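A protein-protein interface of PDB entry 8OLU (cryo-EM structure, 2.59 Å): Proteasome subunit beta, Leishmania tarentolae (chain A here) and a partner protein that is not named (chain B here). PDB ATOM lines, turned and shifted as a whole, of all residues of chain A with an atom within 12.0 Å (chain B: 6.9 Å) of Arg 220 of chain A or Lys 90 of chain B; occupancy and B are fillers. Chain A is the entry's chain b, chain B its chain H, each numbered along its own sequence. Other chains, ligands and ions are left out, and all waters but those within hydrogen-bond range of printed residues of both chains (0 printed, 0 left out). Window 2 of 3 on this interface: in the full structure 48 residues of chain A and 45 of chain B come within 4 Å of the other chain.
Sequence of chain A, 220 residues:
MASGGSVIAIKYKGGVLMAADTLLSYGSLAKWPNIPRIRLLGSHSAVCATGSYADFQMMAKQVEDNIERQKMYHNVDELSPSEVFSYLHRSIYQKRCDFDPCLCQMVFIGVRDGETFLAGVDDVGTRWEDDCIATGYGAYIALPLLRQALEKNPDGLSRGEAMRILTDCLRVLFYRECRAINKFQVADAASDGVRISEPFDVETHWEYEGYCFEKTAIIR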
ATOM      1  N   GLU A 209      24.502  20.078 -20.075  1.00  0.00           N
ATOM      2  CA  GLU A 209      24.061  21.446 -20.028  1.00  0.00           C
ATOM      3  C   GLU A 209      23.301  21.763 -21.322  1.00  0.00           C
ATOM      4  O   GLU A 209      22.357  22.543 -21.327  1.00  0.00           O
ATOM      5  CB  GLU A 209      25.310  22.261 -19.748  1.00  0.00           C
ATOM      6  CG  GLU A 209      25.027  23.707 -19.417  1.00  0.00           C
ATOM      7  CD  GLU A 209      24.970  24.670 -20.607  1.00  0.00           C
ATOM      8  OE1 GLU A 209      26.049  24.838 -21.289  1.00  0.00           O
ATOM      9  OE2 GLU A 209      23.854  25.279 -20.837  1.00  0.00           O
ATOM     10  N   GLY A 210      23.619  21.044 -22.396  1.00  0.00           N
ATOM     11  CA  GLY A 210      23.022  21.306 -23.682  1.00  0.00           C
ATOM     12  C   GLY A 210      21.644  20.718 -23.868  1.00  0.00           C
ATOM     13  O   GLY A 210      21.081  20.824 -24.941  1.00  0.00           O
ATOM     14  N   CYS A 212      19.330  21.372 -21.735  1.00  0.00           N
ATOM     15  CA  CYS A 212      18.466  22.195 -20.934  1.00  0.00           C
ATOM     16  C   CYS A 212      17.396  22.812 -21.825  1.00  0.00           C
ATOM     17  O   CYS A 212      17.487  22.810 -23.043  1.00  0.00           O
ATOM     18  CB  CYS A 212      19.239  23.257 -20.208  1.00  0.00           C
ATOM     19  SG  CYS A 212      19.611  24.583 -21.353  1.00  0.00           S
ATOM     20  N   PHE A 213      16.318  23.231 -21.197  1.00  0.00           N
ATOM     21  CA  PHE A 213      15.163  23.725 -21.893  1.00  0.00           C
ATOM     22  C   PHE A 213      15.483  24.909 -22.764  1.00  0.00           C
ATOM     23  O   PHE A 213      14.924  25.062 -23.823  1.00  0.00           O
ATOM     24  CB  PHE A 213      14.162  24.168 -20.832  1.00  0.00           C
ATOM     25  CG  PHE A 213      12.758  24.266 -21.334  1.00  0.00           C
ATOM     26  CD1 PHE A 213      12.351  25.372 -22.054  1.00  0.00           C
ATOM     27  CD2 PHE A 213      11.892  23.186 -21.179  1.00  0.00           C
ATOM     28  CE1 PHE A 213      11.070  25.444 -22.544  1.00  0.00           C
ATOM     29  CE2 PHE A 213      10.600  23.273 -21.689  1.00  0.00           C
ATOM     30  CZ  PHE A 213      10.203  24.394 -22.378  1.00  0.00           C
ATOM     31  N   GLU A 214      16.296  25.821 -22.255  1.00  0.00           N
ATOM     32  CA  GLU A 214      16.594  27.045 -22.965  1.00  0.00           C
ATOM     33  C   GLU A 214      17.352  26.708 -24.247  1.00  0.00           C
ATOM     34  O   GLU A 214      17.038  27.235 -25.309  1.00  0.00           O
ATOM     35  CB  GLU A 214      17.345  27.981 -22.040  1.00  0.00           C
ATOM     36  CG  GLU A 214      17.560  29.349 -22.681  1.00  0.00           C
ATOM     37  CD  GLU A 214      18.286  30.422 -21.860  1.00  0.00           C
ATOM     38  OE1 GLU A 214      17.665  30.997 -20.913  1.00  0.00           O
ATOM     39  OE2 GLU A 214      19.477  30.702 -22.172  1.00  0.00           O
ATOM     40  N   LYS A 215      18.326  25.806 -24.182  1.00  0.00           N
ATOM     41  CA  LYS A 215      19.160  25.526 -25.341  1.00  0.00           C
ATOM     42  C   LYS A 215      18.422  24.742 -26.420  1.00  0.00           C
ATOM     43  O   LYS A 215      18.479  25.010 -27.596  1.00  0.00           O
ATOM     44  CB  LYS A 215      20.380  24.760 -24.872  1.00  0.00           C
ATOM     45  CG  LYS A 215      21.466  25.625 -24.244  1.00  0.00           C
ATOM     46  CD  LYS A 215      22.684  25.764 -25.187  1.00  0.00           C
ATOM     47  CE  LYS A 215      23.721  26.768 -24.734  1.00  0.00           C
ATOM     48  NZ  LYS A 215      24.296  26.362 -23.428  1.00  0.00           N
ATOM     49  N   THR A 216      17.626  23.800 -26.022  1.00  0.00           N
ATOM     50  CA  THR A 216      16.973  22.948 -26.985  1.00  0.00           C
ATOM     51  C   THR A 216      15.686  23.553 -27.536  1.00  0.00           C
ATOM     52  O   THR A 216      15.088  22.959 -28.432  1.00  0.00           O
ATOM     53  CB  THR A 216      16.701  21.628 -26.283  1.00  0.00           C
ATOM     54  OG1 THR A 216      15.913  21.922 -25.141  1.00  0.00           O
ATOM     55  CG2 THR A 216      17.978  20.983 -25.831  1.00  0.00           C
ATOM     56  N   ALA A 217      15.222  24.652 -26.947  1.00  0.00           N
ATOM     57  CA  ALA A 217      14.106  25.401 -27.494  1.00  0.00           C
ATOM     58  C   ALA A 217      14.317  25.784 -28.951  1.00  0.00           C
ATOM     59  O   ALA A 217      15.397  26.179 -29.348  1.00  0.00           O
ATOM     60  CB  ALA A 217      13.906  26.631 -26.679  1.00  0.00           C
ATOM     61  N   ILE A 218      13.272  25.622 -29.736  1.00  0.00           N
ATOM     62  CA  ILE A 218      13.280  25.869 -31.167  1.00  0.00           C
ATOM     63  C   ILE A 218      13.166  27.354 -31.429  1.00  0.00           C
ATOM     64  O   ILE A 218      13.685  27.820 -32.433  1.00  0.00           O
ATOM     65  CB  ILE A 218      12.105  25.092 -31.801  1.00  0.00           C
ATOM     66  CG1 ILE A 218      12.275  23.572 -31.606  1.00  0.00           C
ATOM     67  CG2 ILE A 218      11.874  25.426 -33.259  1.00  0.00           C
ATOM     68  CD1 ILE A 218      13.571  23.036 -32.147  1.00  0.00           C
ATOM     69  N   ILE A 219      12.500  28.075 -30.531  1.00  0.00           N
ATOM     70  CA  ILE A 219      12.197  29.486 -30.685  1.00  0.00           C
ATOM     71  C   ILE A 219      12.543  30.240 -29.419  1.00  0.00           C
ATOM     72  O   ILE A 219      12.165  29.806 -28.334  1.00  0.00           O
ATOM     73  CB  ILE A 219      10.708  29.618 -30.978  1.00  0.00           C
ATOM     74  CG1 ILE A 219      10.340  29.005 -32.330  1.00  0.00           C
ATOM     75  CG2 ILE A 219      10.240  31.050 -30.854  1.00  0.00           C
ATOM     76  CD1 ILE A 219       8.841  28.890 -32.560  1.00  0.00           C
ATOM     77  N   ARG A 220      13.266  31.359 -29.596  1.00  0.00           N
ATOM     78  CA  ARG A 220      13.763  32.208 -28.516  1.00  0.00           C
ATOM     79  C   ARG A 220      12.682  33.232 -28.078  1.00  0.00           C
ATOM     80  O   ARG A 220      12.568  33.485 -26.841  1.00  0.00           O
ATOM     81  CB  ARG A 220      15.032  32.942 -28.970  1.00  0.00           C
ATOM     82  CG  ARG A 220      16.155  32.067 -29.514  1.00  0.00           C
ATOM     83  CD  ARG A 220      17.034  31.466 -28.425  1.00  0.00           C
ATOM     84  NE  ARG A 220      18.191  30.727 -28.951  1.00  0.00           N
ATOM     85  CZ  ARG A 220      19.262  31.272 -29.534  1.00  0.00           C
ATOM     86  NH1 ARG A 220      20.209  30.502 -30.051  1.00  0.00           N
ATOM     87  NH2 ARG A 220      19.376  32.590 -29.599  1.00  0.00           N
ATOM     88  OXT ARG A 220      11.974  33.762 -28.976  1.00  0.00           O
ATOM     89  N   LEU B  88       8.111  21.485 -26.477  1.00  0.00           N
ATOM     90  CA  LEU B  88       7.370  22.616 -26.001  1.00  0.00           C
ATOM     91  C   LEU B  88       7.926  23.891 -26.559  1.00  0.00           C
ATOM     92  O   LEU B  88       8.927  24.377 -26.076  1.00  0.00           O
ATOM     93  CB  LEU B  88       7.496  22.616 -24.495  1.00  0.00           C
ATOM     94  CG  LEU B  88       7.033  21.308 -23.889  1.00  0.00           C
ATOM     95  CD1 LEU B  88       6.931  21.434 -22.432  1.00  0.00           C
ATOM     96  CD2 LEU B  88       5.649  20.981 -24.381  1.00  0.00           C
ATOM     97  N   THR B  89       7.241  24.444 -27.535  1.00  0.00           N
ATOM     98  CA  THR B  89       7.787  25.484 -28.374  1.00  0.00           C
ATOM     99  C   THR B  89       7.080  26.767 -28.087  1.00  0.00           C
ATOM    100  O   THR B  89       5.906  26.764 -28.099  1.00  0.00           O
ATOM    101  CB  THR B  89       7.654  25.049 -29.822  1.00  0.00           C
ATOM    102  OG1 THR B  89       8.558  23.933 -29.912  1.00  0.00           O
ATOM    103  CG2 THR B  89       8.101  26.109 -30.783  1.00  0.00           C
ATOM    104  N   LYS B  90       7.797  27.827 -27.859  1.00  0.00           N
ATOM    105  CA  LYS B  90       7.227  29.074 -27.427  1.00  0.00           C
ATOM    106  C   LYS B  90       6.548  29.777 -28.612  1.00  0.00           C
ATOM    107  O   LYS B  90       7.089  29.815 -29.701  1.00  0.00           O
ATOM    108  CB  LYS B  90       8.357  29.888 -26.812  1.00  0.00           C
ATOM    109  CG  LYS B  90       8.030  31.356 -26.683  1.00  0.00           C
ATOM    110  CD  LYS B  90       9.038  32.143 -25.898  1.00  0.00           C
ATOM    111  CE  LYS B  90       9.032  33.591 -26.376  1.00  0.00           C
ATOM    112  NZ  LYS B  90       9.146  34.590 -25.256  1.00  0.00           N
ATOM    113  N   LEU B  91       5.332  30.275 -28.459  1.00  0.00           N
ATOM    114  CA  LEU B  91       4.731  31.008 -29.542  1.00  0.00           C
ATOM    115  C   LEU B  91       4.780  32.473 -29.187  1.00  0.00           C
ATOM    116  O   LEU B  91       5.242  33.266 -29.990  1.00  0.00           O
ATOM    117  CB  LEU B  91       3.294  30.576 -29.786  1.00  0.00           C
ATOM    118  CG  LEU B  91       3.149  29.141 -30.249  1.00  0.00           C
ATOM    119  CD1 LEU B  91       1.692  28.819 -30.545  1.00  0.00           C
ATOM    120  CD2 LEU B  91       3.973  28.894 -31.493  1.00  0.00           C
ATOM    121  N   THR B  92       4.284  32.811 -28.012  1.00  0.00           N
ATOM    122  CA  THR B  92       4.511  34.104 -27.408  1.00  0.00           C
ATOM    123  C   THR B  92       5.044  33.916 -26.001  1.00  0.00           C
ATOM    124  O   THR B  92       5.409  32.821 -25.623  1.00  0.00           O
ATOM    125  CB  THR B  92       3.246  34.943 -27.329  1.00  0.00           C
ATOM    126  OG1 THR B  92       2.441  34.458 -26.246  1.00  0.00           O
ATOM    127  CG2 THR B  92       2.490  34.965 -28.647  1.00  0.00           C
ATOM    128  N   LYS B  93       5.073  34.965 -25.205  1.00  0.00           N
ATOM    129  CA  LYS B  93       5.608  34.789 -23.876  1.00  0.00           C
ATOM    130  C   LYS B  93       4.872  33.679 -23.122  1.00  0.00           C
ATOM    131  O   LYS B  93       5.540  32.834 -22.510  1.00  0.00           O
ATOM    132  CB  LYS B  93       5.531  36.063 -23.031  1.00  0.00           C
ATOM    133  CG  LYS B  93       6.435  35.882 -21.831  1.00  0.00           C
ATOM    134  CD  LYS B  93       6.766  37.110 -21.036  1.00  0.00           C
ATOM    135  CE  LYS B  93       7.839  36.741 -20.025  1.00  0.00           C
ATOM    136  NZ  LYS B  93       7.489  37.254 -18.676  1.00  0.00           N
ATOM    137  N   LYS B  94       3.528  33.781 -23.097  1.00  0.00           N
ATOM    138  CA  LYS B  94       2.700  32.881 -22.329  1.00  0.00           C
ATOM    139  C   LYS B  94       1.851  31.965 -23.201  1.00  0.00           C
ATOM    140  O   LYS B  94       0.794  31.575 -22.811  1.00  0.00           O
ATOM    141  CB  LYS B  94       1.685  33.643 -21.518  1.00  0.00           C
ATOM    142  CG  LYS B  94       2.222  34.687 -20.570  1.00  0.00           C
ATOM    143  CD  LYS B  94       2.976  34.103 -19.434  1.00  0.00           C
ATOM    144  CE  LYS B  94       3.393  35.161 -18.419  1.00  0.00           C
ATOM    145  NZ  LYS B  94       2.226  35.699 -17.658  1.00  0.00           N
ATOM    146  N   ILE B  95       2.294  31.602 -24.377  1.00  0.00           N
ATOM    147  CA  ILE B  95       1.544  30.686 -25.178  1.00  0.00           C
ATOM    148  C   ILE B  95       2.511  29.780 -25.890  1.00  0.00           C
ATOM    149  O   ILE B  95       3.455  30.242 -26.480  1.00  0.00           O
ATOM    150  CB  ILE B  95       0.731  31.465 -26.204  1.00  0.00           C
ATOM    151  CG1 ILE B  95      -0.200  32.472 -25.573  1.00  0.00           C
ATOM    152  CG2 ILE B  95      -0.075  30.537 -27.099  1.00  0.00           C
ATOM    153  CD1 ILE B  95      -0.954  33.219 -26.664  1.00  0.00           C
ATOM    154  N   TYR B  96       2.283  28.499 -25.761  1.00  0.00           N
ATOM    155  CA  TYR B  96       3.216  27.495 -26.192  1.00  0.00           C
ATOM    156  C   TYR B  96       2.478  26.503 -27.038  1.00  0.00           C
ATOM    157  O   TYR B  96       1.280  26.463 -27.065  1.00  0.00           O
ATOM    158  CB  TYR B  96       3.871  26.846 -24.999  1.00  0.00           C
ATOM    159  CG  TYR B  96       5.108  27.511 -24.501  1.00  0.00           C
ATOM    160  CD1 TYR B  96       5.055  28.744 -23.933  1.00  0.00           C
ATOM    161  CD2 TYR B  96       6.365  26.920 -24.634  1.00  0.00           C
ATOM    162  CE1 TYR B  96       6.188  29.399 -23.515  1.00  0.00           C
ATOM    163  CE2 TYR B  96       7.542  27.541 -24.192  1.00  0.00           C
ATOM    164  CZ  TYR B  96       7.435  28.807 -23.626  1.00  0.00           C
ATOM    165  OH  TYR B  96       8.509  29.531 -23.175  1.00  0.00           O
ATOM    166  N   CYS B  97       3.201  25.793 -27.840  1.00  0.00           N
ATOM    167  CA  CYS B  97       2.581  24.650 -28.424  1.00  0.00           C
ATOM    168  C   CYS B  97       3.317  23.391 -27.990  1.00  0.00           C
ATOM    169  O   CYS B  97       4.405  23.466 -27.480  1.00  0.00           O
ATOM    170  CB  CYS B  97       2.438  24.803 -29.914  1.00  0.00           C
ATOM    171  SG  CYS B  97       4.014  24.980 -30.732  1.00  0.00           S
ATOM    172  N   ALA B 110       5.388  26.256 -36.192  1.00  0.00           N
ATOM    173  CA  ALA B 110       5.471  26.965 -34.952  1.00  0.00           C
ATOM    174  C   ALA B 110       6.227  28.254 -35.226  1.00  0.00           C
ATOM    175  O   ALA B 110       5.940  29.259 -34.608  1.00  0.00           O
ATOM    176  CB  ALA B 110       6.149  26.077 -33.926  1.00  0.00           C
ATOM    177  N   GLU B 111       7.228  28.217 -36.112  1.00  0.00           N
ATOM    178  CA  GLU B 111       8.076  29.378 -36.302  1.00  0.00           C
ATOM    179  C   GLU B 111       7.245  30.405 -37.044  1.00  0.00           C
ATOM    180  O   GLU B 111       7.291  31.579 -36.750  1.00  0.00           O
ATOM    181  CB  GLU B 111       9.335  29.029 -37.078  1.00  0.00           C
ATOM    182  CG  GLU B 111      10.491  28.566 -36.195  1.00  0.00           C
ATOM    183  CD  GLU B 111      11.552  27.558 -36.724  1.00  0.00           C
ATOM    184  OE1 GLU B 111      11.424  27.007 -37.909  1.00  0.00           O
ATOM    185  OE2 GLU B 111      12.540  27.275 -35.926  1.00  0.00           O
ATOM    186  N   SER B 114       4.592  31.771 -34.616  1.00  0.00           N
ATOM    187  CA  SER B 114       5.160  32.625 -33.600  1.00  0.00           C
ATOM    188  C   SER B 114       5.496  33.985 -34.180  1.00  0.00           C
ATOM    189  O   SER B 114       5.436  34.993 -33.514  1.00  0.00           O
ATOM    190  CB  SER B 114       6.376  31.996 -33.097  1.00  0.00           C
ATOM    191  OG  SER B 114       6.941  32.708 -32.011  1.00  0.00           O
ATOM    192  N   ILE B 231       6.259  22.975 -18.855  1.00  0.00           N
ATOM    193  CA  ILE B 231       6.259  24.381 -18.567  1.00  0.00           C
ATOM    194  C   ILE B 231       4.918  24.726 -18.034  1.00  0.00           C
ATOM    195  O   ILE B 231       4.006  24.096 -18.420  1.00  0.00           O
ATOM    196  CB  ILE B 231       6.673  25.164 -19.813  1.00  0.00           C
ATOM    197  CG1 ILE B 231       6.853  26.628 -19.489  1.00  0.00           C
ATOM    198  CG2 ILE B 231       5.716  25.024 -20.963  1.00  0.00           C
ATOM    199  CD1 ILE B 231       7.436  27.395 -20.675  1.00  0.00           C
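The chain-end carboxylate (O) of Arg 220 of chain A lies within salt-bridge range of the side-chain amino group (NZ) of Lys 90 of chain B (3.9 Å).
The backbone carbonyl oxygen (O) of Thr 89 of chain B sits at hydrogen-bond distance from the backbone NH (N) of Cys 97 of chain B.
O of Leu 91 of chain B lies within hydrogen-bond range of OG of Ser 114 of chain B.
Phe 213 of chain A touches Leu 88 of chain B (CZ to CB, 3.9 Å).
Ile 218 of chain A touches Glu 111 of chain B (CG2 to OE2, 3.3 Å).
CD1 of Ile 219 of chain A touches CG2 of Thr 89 of chain B (3.4 Å).
CD1 of Ile 219 of chain A touches O of Lys 90 of chain B (3.5 Å).
Ile 219 of chain A touches Ala 110 of chain B (CD1 to O, 3.6 Å).
Ile 219 of chain A touches Glu 111 of chain B.
Ser 114 of chain B touches Ile 219 of chain A.
Glu 209 of chain A touches none of the printed residues of chain B.
Of the printed residues of chain B, Ile 218 of chain A touches Glu 111.
Of the printed residues of chain B, Ile 219 of chain A touches Thr 89, Lys 90, Ala 110, Glu 111 and Ser 114.
Arg 220 of chain A touches just one residue of chain B: Lys 90.
Printed residues of chain A within 4 Å of Leu 88 of chain B: Phe 213 (3.9 Å).
Of chain A, only Ile 219 (3.4 Å) comes within 4 Å of Thr 89 of chain B.
Lys 90 of chain B touches just these residues of chain A: Ile 219 (3.5 Å) and Arg 220 (3.6 Å).
No residue of chain A comes within 4 Å of Leu 91 of chain B.
Thr 92 of chain B touches none of the printed residues of chain A.
No residue of chain A comes within 4 Å of Tyr 96 of chain B.
Ala 110 of chain B touches just one residue of chain A: Ile 219 (3.6 Å).
The nearest residue of chain B that does not touch Arg 220 of chain A is Ser 114 of chain B (6.0 Å).
The nearest printed residue of chain A that does not touch Leu 88 of chain B is Ala 217 of chain A (5.5 Å).
Of the 11 printed residues of chain A, 4 touch a printed residue of chain B.
Hydrophobic or aromatic side chains of chain A within 4 Å of the printed part of chain B: Phe 213, Ile 218 and Ile 219.
Of the 14 printed residues of chain B, 6 touch a printed residue of chain A.
Hydrophobic or aromatic side chains of chain B within 4 Å of the printed part of chain A: Leu 88.
Among the printed residues, no Asp or Glu carboxylate lies within 4 Å of a Lys or Arg side-chain nitrogen of the other chain.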
